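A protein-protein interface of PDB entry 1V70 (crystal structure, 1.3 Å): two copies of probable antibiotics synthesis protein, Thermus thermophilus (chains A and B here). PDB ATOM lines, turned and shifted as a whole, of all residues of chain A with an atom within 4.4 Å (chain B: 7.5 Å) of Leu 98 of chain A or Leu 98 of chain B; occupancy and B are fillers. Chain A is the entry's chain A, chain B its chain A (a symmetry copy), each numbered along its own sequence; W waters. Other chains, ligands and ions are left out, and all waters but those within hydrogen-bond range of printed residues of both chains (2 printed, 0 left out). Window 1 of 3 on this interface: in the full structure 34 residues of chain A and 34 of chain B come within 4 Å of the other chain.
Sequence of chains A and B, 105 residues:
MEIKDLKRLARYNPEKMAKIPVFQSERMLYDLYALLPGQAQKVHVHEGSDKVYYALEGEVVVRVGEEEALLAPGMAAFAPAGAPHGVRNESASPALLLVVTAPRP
The backbone carbonyl oxygen (O) of Tyr 30 of chain B lies within hydrogen-bond range of the backbone NH (N) of Val 22 of chain B, at 2.9 Å.
O of Val 100 of chain B sits at hydrogen-bond distance from N of Val 52 of chain B (2.9 Å).
O of Val 100 of chain A lies within hydrogen-bond range of N of Val 52 of chain A, 2.9 Å away.
O of Tyr 54 of chain B is in hydrogen-bond range of N of Leu 98 of chain B.
The backbone carbonyl oxygen (O) of Tyr 54 of chain A is in hydrogen-bond range of the backbone NH (N) of Leu 98 of chain A (2.8 Å).
Leu 6 of chain A touches Tyr 54 of chain B.
Ala 76 of chain B touches Leu 6 of chain A.
Tyr 30 of chain A touches Val 52 of chain B.
Tyr 54 of chain B touches Tyr 30 of chain A (CB to OH, 3.3 Å).
CD2 of Leu 6 of chain B touches CE1 of Tyr 54 of chain A (3.4 Å).
CB of Tyr 54 of chain A touches OH of Tyr 30 of chain B, at 3.3 Å.
Leu 56 of chain B touches Tyr 54 of chain A (CD2 to OH, 3.5 Å).
OH of Tyr 54 of chain B touches CD2 of Leu 56 of chain A, 3.5 Å away.
CD2 of Leu 98 of chain B touches CD2 of Leu 98 of chain A (3.9 Å).
Of the printed residues of chain B, Leu 56 of chain A touches Tyr 54 (3.5 Å).
Of the printed residues of chain B, Leu 98 of chain A touches Leu 98 (3.9 Å).
Of the printed residues of chain A, Leu 6 of chain B touches Tyr 54 (3.4 Å).
Tyr 53 of chain B touches none of the printed residues of chain A.
Printed residues of chain A within 4 Å of Leu 56 of chain B: Tyr 54 (3.5 Å).
Leu 71 of chain B touches none of the printed residues of chain A.
Of the printed residues of chain A, Leu 98 of chain B touches Leu 98.
The nearest residue of chain B that does not touch Leu 98 of chain A is Tyr 54 of chain B (4.4 Å).
Of the 12 printed residues of chain A, 7 touch a printed residue of chain B.
Hydrophobic or aromatic side chains of chain A that line the printed part of chain B: Leu 6, Tyr 30, Val 52, Tyr 54, Leu 56, Leu 98 and Val 100.
Of the 24 printed residues of chain B, 8 touch a printed residue of chain A.
Hydrophobic or aromatic side chains of chain B within 4 Å of the printed part of chain A: Leu 6, Tyr 30, Val 52, Tyr 54, Leu 56, Ala 76, Leu 98 and Val 100.
Among the printed residues, 11 pairs touch across the chains.
Tyr 30 of chain A touches Val 52 of chain B, and with the chains exchanged Val 52 of chain A touches Tyr 30 of chain B.
Tyr 30 of chain A touches Tyr 54 of chain B, and with the chains exchanged Tyr 54 of chain A touches Tyr 30 of chain B.
Tyr 54 of chain A touches Leu 56 of chain B, and with the chains exchanged Leu 56 of chain A touches Tyr 54 of chain B.
Val 100 of chain A touches its own counterpart, Val 100 of chain B.
Of the 11 pairs that touch across the chains among the printed residues, 10 have their exchanged pair printed and touching as well.
Water W2 lies within hydrogen-bond range of the side-chain hydroxyl (OH) of Tyr 30 of chain B, the backbone carbonyl oxygen (O) of Leu 98 of chain A and the backbone carbonyl oxygen (O) of Val 52 of chain A.
Water W1 lies within hydrogen-bond range of OH of Tyr 30 of chain A, O of Leu 98 of chain B and O of Val 52 of chain B.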
ATOM      1  N   LEU A   6       1.104  33.234  24.295  1.00  0.00           N
ATOM      2  CA  LEU A   6       1.116  31.814  24.623  1.00  0.00           C
ATOM      3  C   LEU A   6       1.930  31.485  25.866  1.00  0.00           C
ATOM      4  O   LEU A   6       1.636  30.512  26.565  1.00  0.00           O
ATOM      5  CB  LEU A   6       1.622  30.997  23.430  1.00  0.00           C
ATOM      6  CG  LEU A   6       0.606  30.728  22.312  1.00  0.00           C
ATOM      7  CD1 LEU A   6      -0.002  32.025  21.807  1.00  0.00           C
ATOM      8  CD2 LEU A   6       1.293  29.976  21.183  1.00  0.00           C
ATOM      9  N   TYR A  30      -6.442  25.572  17.520  1.00  0.00           N
ATOM     10  CA  TYR A  30      -5.093  26.091  17.720  1.00  0.00           C
ATOM     11  C   TYR A  30      -4.912  25.963  19.225  1.00  0.00           C
ATOM     12  O   TYR A  30      -5.433  26.775  19.996  1.00  0.00           O
ATOM     13  CB  TYR A  30      -5.042  27.555  17.276  1.00  0.00           C
ATOM     14  CG  TYR A  30      -3.657  28.093  16.993  1.00  0.00           C
ATOM     15  CD1 TYR A  30      -3.071  27.960  15.729  1.00  0.00           C
ATOM     16  CD2 TYR A  30      -2.943  28.763  17.980  1.00  0.00           C
ATOM     17  CE1 TYR A  30      -1.804  28.493  15.462  1.00  0.00           C
ATOM     18  CE2 TYR A  30      -1.686  29.296  17.726  1.00  0.00           C
ATOM     19  CZ  TYR A  30      -1.123  29.162  16.466  1.00  0.00           C
ATOM     20  OH  TYR A  30       0.109  29.727  16.225  1.00  0.00           O
ATOM     21  N   ASP A  31      -4.186  24.926  19.638  1.00  0.00           N
ATOM     22  CA  ASP A  31      -3.994  24.627  21.054  1.00  0.00           C
ATOM     23  C   ASP A  31      -2.557  24.503  21.511  1.00  0.00           C
ATOM     24  O   ASP A  31      -1.630  24.399  20.711  1.00  0.00           O
ATOM     25  CB  ASP A  31      -4.645  23.280  21.403  1.00  0.00           C
ATOM     26  CG  ASP A  31      -6.082  23.179  20.962  1.00  0.00           C
ATOM     27  OD1 ASP A  31      -6.850  24.116  21.231  1.00  0.00           O
ATOM     28  OD2 ASP A  31      -6.446  22.143  20.358  1.00  0.00           O
ATOM     29  N   LEU A  32      -2.399  24.494  22.829  1.00  0.00           N
ATOM     30  CA  LEU A  32      -1.111  24.259  23.452  1.00  0.00           C
ATOM     31  C   LEU A  32      -1.307  22.948  24.207  1.00  0.00           C
ATOM     32  O   LEU A  32      -2.344  22.749  24.846  1.00  0.00           O
ATOM     33  CB  LEU A  32      -0.755  25.344  24.471  1.00  0.00           C
ATOM     34  CG  LEU A  32      -0.364  26.740  23.997  1.00  0.00           C
ATOM     35  CD1 LEU A  32      -0.062  27.603  25.217  1.00  0.00           C
ATOM     36  CD2 LEU A  32       0.852  26.665  23.082  1.00  0.00           C
ATOM     37  N   VAL A  52      -0.755  19.014  13.204  1.00  0.00           N
ATOM     38  CA  VAL A  52       0.671  19.301  13.213  1.00  0.00           C
ATOM     39  C   VAL A  52       1.107  19.631  14.636  1.00  0.00           C
ATOM     40  O   VAL A  52       0.486  20.461  15.310  1.00  0.00           O
ATOM     41  CB  VAL A  52       1.044  20.501  12.310  1.00  0.00           C
ATOM     42  CG1 VAL A  52       2.543  20.778  12.406  1.00  0.00           C
ATOM     43  CG2 VAL A  52       0.658  20.212  10.868  1.00  0.00           C
ATOM     44  N   TYR A  53       2.158  18.956  15.091  1.00  0.00           N
ATOM     45  CA  TYR A  53       2.733  19.176  16.416  1.00  0.00           C
ATOM     46  C   TYR A  53       4.009  19.991  16.234  1.00  0.00           C
ATOM     47  O   TYR A  53       4.831  19.663  15.376  1.00  0.00           O
ATOM     48  CB  TYR A  53       3.152  17.857  17.068  1.00  0.00           C
ATOM     49  CG  TYR A  53       2.048  16.877  17.377  1.00  0.00           C
ATOM     50  CD1 TYR A  53       1.233  17.035  18.499  1.00  0.00           C
ATOM     51  CD2 TYR A  53       1.868  15.745  16.587  1.00  0.00           C
ATOM     52  CE1 TYR A  53       0.273  16.081  18.829  1.00  0.00           C
ATOM     53  CE2 TYR A  53       0.913  14.789  16.906  1.00  0.00           C
ATOM     54  CZ  TYR A  53       0.124  14.959  18.028  1.00  0.00           C
ATOM     55  OH  TYR A  53      -0.793  13.988  18.360  1.00  0.00           O
ATOM     56  N   TYR A  54       4.181  21.038  17.033  1.00  0.00           N
ATOM     57  CA  TYR A  54       5.391  21.860  16.984  1.00  0.00           C
ATOM     58  C   TYR A  54       5.913  21.966  18.416  1.00  0.00           C
ATOM     59  O   TYR A  54       5.168  22.334  19.327  1.00  0.00           O
ATOM     60  CB  TYR A  54       5.091  23.257  16.438  1.00  0.00           C
ATOM     61  CG  TYR A  54       6.280  24.195  16.518  1.00  0.00           C
ATOM     62  CD1 TYR A  54       7.371  24.046  15.663  1.00  0.00           C
ATOM     63  CD2 TYR A  54       6.327  25.212  17.472  1.00  0.00           C
ATOM     64  CE1 TYR A  54       8.483  24.887  15.758  1.00  0.00           C
ATOM     65  CE2 TYR A  54       7.432  26.056  17.575  1.00  0.00           C
ATOM     66  CZ  TYR A  54       8.504  25.888  16.715  1.00  0.00           C
ATOM     67  OH  TYR A  54       9.594  26.725  16.804  1.00  0.00           O
ATOM     68  N   LEU A  56       7.633  23.637  21.406  1.00  0.00           N
ATOM     69  CA  LEU A  56       7.995  24.958  21.913  1.00  0.00           C
ATOM     70  C   LEU A  56       9.068  24.824  22.990  1.00  0.00           C
ATOM     71  O   LEU A  56      10.026  25.597  23.029  1.00  0.00           O
ATOM     72  CB  LEU A  56       6.769  25.655  22.509  1.00  0.00           C
ATOM     73  CG  LEU A  56       5.646  26.036  21.543  1.00  0.00           C
ATOM     74  CD1 LEU A  56       4.396  26.391  22.337  1.00  0.00           C
ATOM     75  CD2 LEU A  56       6.090  27.201  20.667  1.00  0.00           C
ATOM     76  N   LEU A  97       3.831  21.996  23.589  1.00  0.00           N
ATOM     77  CA  LEU A  97       3.666  21.915  22.143  1.00  0.00           C
ATOM     78  C   LEU A  97       2.583  22.852  21.650  1.00  0.00           C
ATOM     79  O   LEU A  97       1.618  23.120  22.364  1.00  0.00           O
ATOM     80  CB  LEU A  97       3.256  20.497  21.734  1.00  0.00           C
ATOM     81  CG  LEU A  97       4.015  19.323  22.348  1.00  0.00           C
ATOM     82  CD1 LEU A  97       3.366  18.021  21.909  1.00  0.00           C
ATOM     83  CD2 LEU A  97       5.475  19.385  21.934  1.00  0.00           C
ATOM     84  N   LEU A  98       2.763  23.353  20.434  1.00  0.00           N
ATOM     85  CA  LEU A  98       1.767  24.178  19.769  1.00  0.00           C
ATOM     86  C   LEU A  98       1.178  23.145  18.808  1.00  0.00           C
ATOM     87  O   LEU A  98       1.901  22.565  17.983  1.00  0.00           O
ATOM     88  CB  LEU A  98       2.424  25.328  19.007  1.00  0.00           C
ATOM     89  CG  LEU A  98       1.482  26.212  18.182  1.00  0.00           C
ATOM     90  CD1 LEU A  98       0.379  26.780  19.059  1.00  0.00           C
ATOM     91  CD2 LEU A  98       2.283  27.331  17.539  1.00  0.00           C
ATOM     92  N   VAL A  99      -0.121  22.896  18.931  1.00  0.00           N
ATOM     93  CA  VAL A  99      -0.789  21.883  18.123  1.00  0.00           C
ATOM     94  C   VAL A  99      -1.944  22.458  17.324  1.00  0.00           C
ATOM     95  O   VAL A  99      -2.832  23.110  17.881  1.00  0.00           O
ATOM     96  CB  VAL A  99      -1.326  20.747  19.029  1.00  0.00           C
ATOM     97  CG1 VAL A  99      -1.832  19.587  18.185  1.00  0.00           C
ATOM     98  CG2 VAL A  99      -0.235  20.287  19.984  1.00  0.00           C
ATOM     99  N   VAL A 100      -1.931  22.208  16.021  1.00  0.00           N
ATOM    100  CA  VAL A 100      -2.978  22.701  15.138  1.00  0.00           C
ATOM    101  C   VAL A 100      -3.696  21.533  14.479  1.00  0.00           C
ATOM    102  O   VAL A 100      -3.060  20.623  13.943  1.00  0.00           O
ATOM    103  CB  VAL A 100      -2.395  23.607  14.031  1.00  0.00           C
ATOM    104  CG1 VAL A 100      -3.519  24.136  13.144  1.00  0.00           C
ATOM    105  CG2 VAL A 100      -1.623  24.760  14.649  1.00  0.00           C
ATOM    106  N   LEU B   6      12.205  23.552  11.748  1.00  0.00           N
ATOM    107  CA  LEU B   6      11.903  24.883  11.234  1.00  0.00           C
ATOM    108  C   LEU B   6      13.089  25.834  11.279  1.00  0.00           C
ATOM    109  O   LEU B   6      13.190  26.747  10.456  1.00  0.00           O
ATOM    110  CB  LEU B   6      10.713  25.485  11.986  1.00  0.00           C
ATOM    111  CG  LEU B   6       9.323  25.004  11.553  1.00  0.00           C
ATOM    112  CD1 LEU B   6       9.230  23.489  11.607  1.00  0.00           C
ATOM    113  CD2 LEU B   6       8.271  25.643  12.448  1.00  0.00           C
ATOM    114  N   ILE B  20       7.817  30.403   3.265  1.00  0.00           N
ATOM    115  CA  ILE B  20       8.463  29.101   3.275  1.00  0.00           C
ATOM    116  C   ILE B  20       7.494  27.986   3.651  1.00  0.00           C
ATOM    117  O   ILE B  20       7.126  27.848   4.813  1.00  0.00           O
ATOM    118  CB  ILE B  20       9.627  29.128   4.287  1.00  0.00           C
ATOM    119  CG1 ILE B  20      10.572  30.284   3.943  1.00  0.00           C
ATOM    120  CG2 ILE B  20      10.355  27.796   4.296  1.00  0.00           C
ATOM    121  CD1 ILE B  20      11.358  30.818   5.128  1.00  0.00           C
ATOM    122  N   VAL B  22       6.119  24.581   4.880  1.00  0.00           N
ATOM    123  CA  VAL B  22       6.637  23.523   5.737  1.00  0.00           C
ATOM    124  C   VAL B  22       5.846  22.260   5.401  1.00  0.00           C
ATOM    125  O   VAL B  22       6.416  21.255   4.974  1.00  0.00           O
ATOM    126  CB  VAL B  22       6.470  23.881   7.233  1.00  0.00           C
ATOM    127  CG1 VAL B  22       7.046  22.768   8.101  1.00  0.00           C
ATOM    128  CG2 VAL B  22       7.177  25.200   7.535  1.00  0.00           C
ATOM    129  N   LEU B  29      -2.409  25.161   5.369  1.00  0.00           N
ATOM    130  CA  LEU B  29      -1.104  25.611   4.924  1.00  0.00           C
ATOM    131  C   LEU B  29      -0.364  25.863   6.231  1.00  0.00           C
ATOM    132  O   LEU B  29      -0.891  26.510   7.136  1.00  0.00           O
ATOM    133  CB  LEU B  29      -1.194  26.914   4.131  1.00  0.00           C
ATOM    134  CG  LEU B  29      -1.848  26.858   2.750  1.00  0.00           C
ATOM    135  CD1 LEU B  29      -1.750  28.230   2.105  1.00  0.00           C
ATOM    136  CD2 LEU B  29      -1.159  25.810   1.883  1.00  0.00           C
ATOM    137  N   TYR B  30       0.841  25.320   6.339  1.00  0.00           N
ATOM    138  CA  TYR B  30       1.660  25.477   7.536  1.00  0.00           C
ATOM    139  C   TYR B  30       2.948  26.063   6.978  1.00  0.00           C
ATOM    140  O   TYR B  30       3.771  25.345   6.402  1.00  0.00           O
ATOM    141  CB  TYR B  30       1.901  24.103   8.169  1.00  0.00           C
ATOM    142  CG  TYR B  30       2.328  24.131   9.619  1.00  0.00           C
ATOM    143  CD1 TYR B  30       1.386  24.153  10.654  1.00  0.00           C
ATOM    144  CD2 TYR B  30       3.676  24.103   9.961  1.00  0.00           C
ATOM    145  CE1 TYR B  30       1.787  24.140  11.995  1.00  0.00           C
ATOM    146  CE2 TYR B  30       4.085  24.090  11.288  1.00  0.00           C
ATOM    147  CZ  TYR B  30       3.138  24.104  12.300  1.00  0.00           C
ATOM    148  OH  TYR B  30       3.562  24.055  13.609  1.00  0.00           O
ATOM    149  N   ASP B  31       3.107  27.375   7.135  1.00  0.00           N
ATOM    150  CA  ASP B  31       4.252  28.091   6.581  1.00  0.00           C
ATOM    151  C   ASP B  31       5.054  28.913   7.565  1.00  0.00           C
ATOM    152  O   ASP B  31       4.629  29.173   8.689  1.00  0.00           O
ATOM    153  CB  ASP B  31       3.784  29.089   5.511  1.00  0.00           C
ATOM    154  CG  ASP B  31       2.902  28.468   4.458  1.00  0.00           C
ATOM    155  OD1 ASP B  31       3.271  27.407   3.931  1.00  0.00           O
ATOM    156  OD2 ASP B  31       1.845  29.061   4.146  1.00  0.00           O
ATOM    157  N   LEU B  32       6.224  29.336   7.104  1.00  0.00           N
ATOM    158  CA  LEU B  32       7.073  30.237   7.858  1.00  0.00           C
ATOM    159  C   LEU B  32       7.113  31.500   7.003  1.00  0.00           C
ATOM    160  O   LEU B  32       7.241  31.415   5.778  1.00  0.00           O
ATOM    161  CB  LEU B  32       8.503  29.709   7.990  1.00  0.00           C
ATOM    162  CG  LEU B  32       8.801  28.529   8.908  1.00  0.00           C
ATOM    163  CD1 LEU B  32      10.293  28.224   8.844  1.00  0.00           C
ATOM    164  CD2 LEU B  32       8.382  28.852  10.336  1.00  0.00           C
ATOM    165  N   TYR B  33       6.958  32.661   7.626  1.00  0.00           N
ATOM    166  CA  TYR B  33       7.062  33.923   6.898  1.00  0.00           C
ATOM    167  C   TYR B  33       8.319  34.569   7.455  1.00  0.00           C
ATOM    168  O   TYR B  33       8.460  34.710   8.669  1.00  0.00           O
ATOM    169  CB  TYR B  33       5.882  34.858   7.172  1.00  0.00           C
ATOM    170  CG  TYR B  33       4.587  34.549   6.453  1.00  0.00           C
ATOM    171  CD1 TYR B  33       3.547  35.479   6.465  1.00  0.00           C
ATOM    172  CD2 TYR B  33       4.374  33.332   5.797  1.00  0.00           C
ATOM    173  CE1 TYR B  33       2.326  35.213   5.852  1.00  0.00           C
ATOM    174  CE2 TYR B  33       3.148  33.053   5.175  1.00  0.00           C
ATOM    175  CZ  TYR B  33       2.131  34.002   5.211  1.00  0.00           C
ATOM    176  OH  TYR B  33       0.910  33.746   4.626  1.00  0.00           O
ATOM    177  N   LYS B  51      -6.741  32.396   9.521  1.00  0.00           N
ATOM    178  CA  LYS B  51      -5.287  32.419   9.568  1.00  0.00           C
ATOM    179  C   LYS B  51      -4.807  32.830  10.950  1.00  0.00           C
ATOM    180  O   LYS B  51      -5.432  33.653  11.616  1.00  0.00           O
ATOM    181  CB  LYS B  51      -4.730  33.389   8.516  1.00  0.00           C
ATOM    182  CG  LYS B  51      -3.210  33.481   8.520  1.00  0.00           C
ATOM    183  CD  LYS B  51      -2.706  34.552   7.571  1.00  0.00           C
ATOM    184  CE  LYS B  51      -3.018  34.208   6.132  1.00  0.00           C
ATOM    185  NZ  LYS B  51      -2.528  35.266   5.210  1.00  0.00           N
ATOM    186  N   VAL B  52      -3.707  32.233  11.390  1.00  0.00           N
ATOM    187  CA  VAL B  52      -3.120  32.574  12.678  1.00  0.00           C
ATOM    188  C   VAL B  52      -1.632  32.844  12.494  1.00  0.00           C
ATOM    189  O   VAL B  52      -0.915  32.044  11.882  1.00  0.00           O
ATOM    190  CB  VAL B  52      -3.276  31.441  13.721  1.00  0.00           C
ATOM    191  CG1 VAL B  52      -2.596  31.844  15.028  1.00  0.00           C
ATOM    192  CG2 VAL B  52      -4.747  31.151  13.965  1.00  0.00           C
ATOM    193  N   TYR B  53      -1.184  33.986  13.005  1.00  0.00           N
ATOM    194  CA  TYR B  53       0.223  34.383  12.956  1.00  0.00           C
ATOM    195  C   TYR B  53       0.815  34.151  14.342  1.00  0.00           C
ATOM    196  O   TYR B  53       0.213  34.548  15.342  1.00  0.00           O
ATOM    197  CB  TYR B  53       0.369  35.879  12.669  1.00  0.00           C
ATOM    198  CG  TYR B  53      -0.127  36.360  11.329  1.00  0.00           C
ATOM    199  CD1 TYR B  53       0.631  36.184  10.170  1.00  0.00           C
ATOM    200  CD2 TYR B  53      -1.325  37.063  11.231  1.00  0.00           C
ATOM    201  CE1 TYR B  53       0.210  36.707   8.950  1.00  0.00           C
ATOM    202  CE2 TYR B  53      -1.755  37.587  10.020  1.00  0.00           C
ATOM    203  CZ  TYR B  53      -0.984  37.411   8.887  1.00  0.00           C
ATOM    204  OH  TYR B  53      -1.397  37.968   7.698  1.00  0.00           O
ATOM    205  N   TYR B  54       1.983  33.521  14.407  1.00  0.00           N
ATOM    206  CA  TYR B  54       2.670  33.291  15.678  1.00  0.00           C
ATOM    207  C   TYR B  54       4.102  33.793  15.505  1.00  0.00           C
ATOM    208  O   TYR B  54       4.790  33.407  14.558  1.00  0.00           O
ATOM    209  CB  TYR B  54       2.684  31.804  16.040  1.00  0.00           C
ATOM    210  CG  TYR B  54       3.522  31.497  17.266  1.00  0.00           C
ATOM    211  CD1 TYR B  54       3.084  31.850  18.542  1.00  0.00           C
ATOM    212  CD2 TYR B  54       4.769  30.884  17.146  1.00  0.00           C
ATOM    213  CE1 TYR B  54       3.869  31.601  19.669  1.00  0.00           C
ATOM    214  CE2 TYR B  54       5.561  30.631  18.265  1.00  0.00           C
ATOM    215  CZ  TYR B  54       5.104  30.992  19.522  1.00  0.00           C
ATOM    216  OH  TYR B  54       5.877  30.735  20.633  1.00  0.00           O
ATOM    217  N   ALA B  55       4.550  34.663  16.404  1.00  0.00           N
ATOM    218  CA  ALA B  55       5.902  35.208  16.304  1.00  0.00           C
ATOM    219  C   ALA B  55       6.965  34.292  16.909  1.00  0.00           C
ATOM    220  O   ALA B  55       6.941  33.998  18.106  1.00  0.00           O
ATOM    221  CB  ALA B  55       5.958  36.592  16.965  1.00  0.00           C
ATOM    222  N   LEU B  56       7.894  33.841  16.066  1.00  0.00           N
ATOM    223  CA  LEU B  56       8.987  32.972  16.498  1.00  0.00           C
ATOM    224  C   LEU B  56      10.195  33.818  16.890  1.00  0.00           C
ATOM    225  O   LEU B  56      10.856  33.549  17.894  1.00  0.00           O
ATOM    226  CB  LEU B  56       9.386  32.019  15.368  1.00  0.00           C
ATOM    227  CG  LEU B  56       8.358  30.967  14.949  1.00  0.00           C
ATOM    228  CD1 LEU B  56       8.778  30.353  13.620  1.00  0.00           C
ATOM    229  CD2 LEU B  56       8.235  29.901  16.031  1.00  0.00           C
ATOM    230  N   GLU B  57      10.482  34.836  16.082  1.00  0.00           N
ATOM    231  CA  GLU B  57      11.634  35.734  16.277  1.00  0.00           C
ATOM    232  C   GLU B  57      11.265  37.131  15.828  1.00  0.00           C
ATOM    233  O   GLU B  57      10.561  37.332  14.848  1.00  0.00           O
ATOM    234  CB  GLU B  57      12.864  35.273  15.473  1.00  0.00           C
ATOM    235  CG  GLU B  57      13.324  33.844  15.755  1.00  0.00           C
ATOM    236  CD  GLU B  57      14.666  33.591  15.080  1.00  0.00           C
ATOM    237  OE1 GLU B  57      14.812  33.960  13.923  1.00  0.00           O
ATOM    238  OE2 GLU B  57      15.545  33.028  15.722  1.00  0.00           O
ATOM    239  N   LEU B  71       3.146  42.157  17.578  1.00  0.00           N
ATOM    240  CA  LEU B  71       3.315  40.745  17.863  1.00  0.00           C
ATOM    241  C   LEU B  71       4.784  40.449  18.152  1.00  0.00           C
ATOM    242  O   LEU B  71       5.622  40.492  17.245  1.00  0.00           O
ATOM    243  CB  LEU B  71       2.835  39.931  16.660  1.00  0.00           C
ATOM    244  CG  LEU B  71       2.412  38.478  16.871  1.00  0.00           C
ATOM    245  CD1 LEU B  71       1.114  38.429  17.679  1.00  0.00           C
ATOM    246  CD2 LEU B  71       2.218  37.812  15.516  1.00  0.00           C
ATOM    247  N   MET B  75       3.766  35.424  20.993  1.00  0.00           N
ATOM    248  CA  MET B  75       2.409  35.931  20.814  1.00  0.00           C
ATOM    249  C   MET B  75       1.793  35.462  19.502  1.00  0.00           C
ATOM    250  O   MET B  75       2.492  35.308  18.495  1.00  0.00           O
ATOM    251  CB  MET B  75       2.405  37.461  20.850  1.00  0.00           C
ATOM    252  CG  MET B  75       2.768  38.054  22.203  1.00  0.00           C
ATOM    253  SD  MET B  75       2.935  39.852  22.170  1.00  0.00           S
ATOM    254  CE  MET B  75       1.236  40.352  21.865  1.00  0.00           C
ATOM    255  N   ALA B  76       0.484  35.239  19.526  1.00  0.00           N
ATOM    256  CA  ALA B  76      -0.256  34.803  18.347  1.00  0.00           C
ATOM    257  C   ALA B  76      -1.488  35.676  18.144  1.00  0.00           C
ATOM    258  O   ALA B  76      -2.105  36.132  19.114  1.00  0.00           O
ATOM    259  CB  ALA B  76      -0.672  33.339  18.499  1.00  0.00           C
ATOM    260  N   ALA B  77      -1.840  35.901  16.883  1.00  0.00           N
ATOM    261  CA  ALA B  77      -3.003  36.704  16.521  1.00  0.00           C
ATOM    262  C   ALA B  77      -3.843  35.927  15.510  1.00  0.00           C
ATOM    263  O   ALA B  77      -3.306  35.312  14.580  1.00  0.00           O
ATOM    264  CB  ALA B  77      -2.561  38.034  15.928  1.00  0.00           C
ATOM    265  N   LEU B  96      10.531  36.366  12.091  1.00  0.00           N
ATOM    266  CA  LEU B  96      10.137  35.058  11.582  1.00  0.00           C
ATOM    267  C   LEU B  96       8.817  34.672  12.231  1.00  0.00           C
ATOM    268  O   LEU B  96       8.685  34.714  13.453  1.00  0.00           O
ATOM    269  CB  LEU B  96      11.187  33.998  11.926  1.00  0.00           C
ATOM    270  CG  LEU B  96      11.012  32.641  11.240  1.00  0.00           C
ATOM    271  CD1 LEU B  96      11.144  32.806   9.730  1.00  0.00           C
ATOM    272  CD2 LEU B  96      12.059  31.671  11.757  1.00  0.00           C
ATOM    273  N   LEU B  97       7.850  34.283  11.406  1.00  0.00           N
ATOM    274  CA  LEU B  97       6.533  33.901  11.896  1.00  0.00           C
ATOM    275  C   LEU B  97       6.150  32.507  11.445  1.00  0.00           C
ATOM    276  O   LEU B  97       6.556  32.066  10.371  1.00  0.00           O
ATOM    277  CB  LEU B  97       5.467  34.860  11.356  1.00  0.00           C
ATOM    278  CG  LEU B  97       5.751  36.358  11.413  1.00  0.00           C
ATOM    279  CD1 LEU B  97       4.631  37.109  10.712  1.00  0.00           C
ATOM    280  CD2 LEU B  97       5.894  36.797  12.860  1.00  0.00           C
ATOM    281  N   LEU B  98       5.377  31.822  12.279  1.00  0.00           N
ATOM    282  CA  LEU B  98       4.829  30.515  11.950  1.00  0.00           C
ATOM    283  C   LEU B  98       3.395  30.918  11.607  1.00  0.00           C
ATOM    284  O   LEU B  98       2.687  31.503  12.441  1.00  0.00           O
ATOM    285  CB  LEU B  98       4.867  29.582  13.159  1.00  0.00           C
ATOM    286  CG  LEU B  98       4.223  28.205  12.963  1.00  0.00           C
ATOM    287  CD1 LEU B  98       4.849  27.487  11.778  1.00  0.00           C
ATOM    288  CD2 LEU B  98       4.395  27.389  14.232  1.00  0.00           C
ATOM    289  N   VAL B  99       2.978  30.632  10.379  1.00  0.00           N
ATOM    290  CA  VAL B  99       1.657  31.026   9.904  1.00  0.00           C
ATOM    291  C   VAL B  99       0.841  29.836   9.433  1.00  0.00           C
ATOM    292  O   VAL B  99       1.297  29.050   8.599  1.00  0.00           O
ATOM    293  CB  VAL B  99       1.787  32.034   8.737  1.00  0.00           C
ATOM    294  CG1 VAL B  99       0.427  32.613   8.378  1.00  0.00           C
ATOM    295  CG2 VAL B  99       2.764  33.139   9.113  1.00  0.00           C
ATOM    296  N   VAL B 100      -0.368  29.713   9.966  1.00  0.00           N
ATOM    297  CA  VAL B 100      -1.256  28.618   9.603  1.00  0.00           C
ATOM    298  C   VAL B 100      -2.530  29.165   8.978  1.00  0.00           C
ATOM    299  O   VAL B 100      -3.157  30.077   9.520  1.00  0.00           O
ATOM    300  CB  VAL B 100      -1.638  27.775  10.839  1.00  0.00           C
ATOM    301  CG1 VAL B 100      -2.538  26.615  10.422  1.00  0.00           C
ATOM    302  CG2 VAL B 100      -0.386  27.251  11.524  1.00  0.00           C
HETATM  303  O   HOH W   1       0.480  30.198  13.558  1.00  0.00           O
HETATM  304  O   HOH W   2       1.604  23.090  15.253  1.00  0.00           O
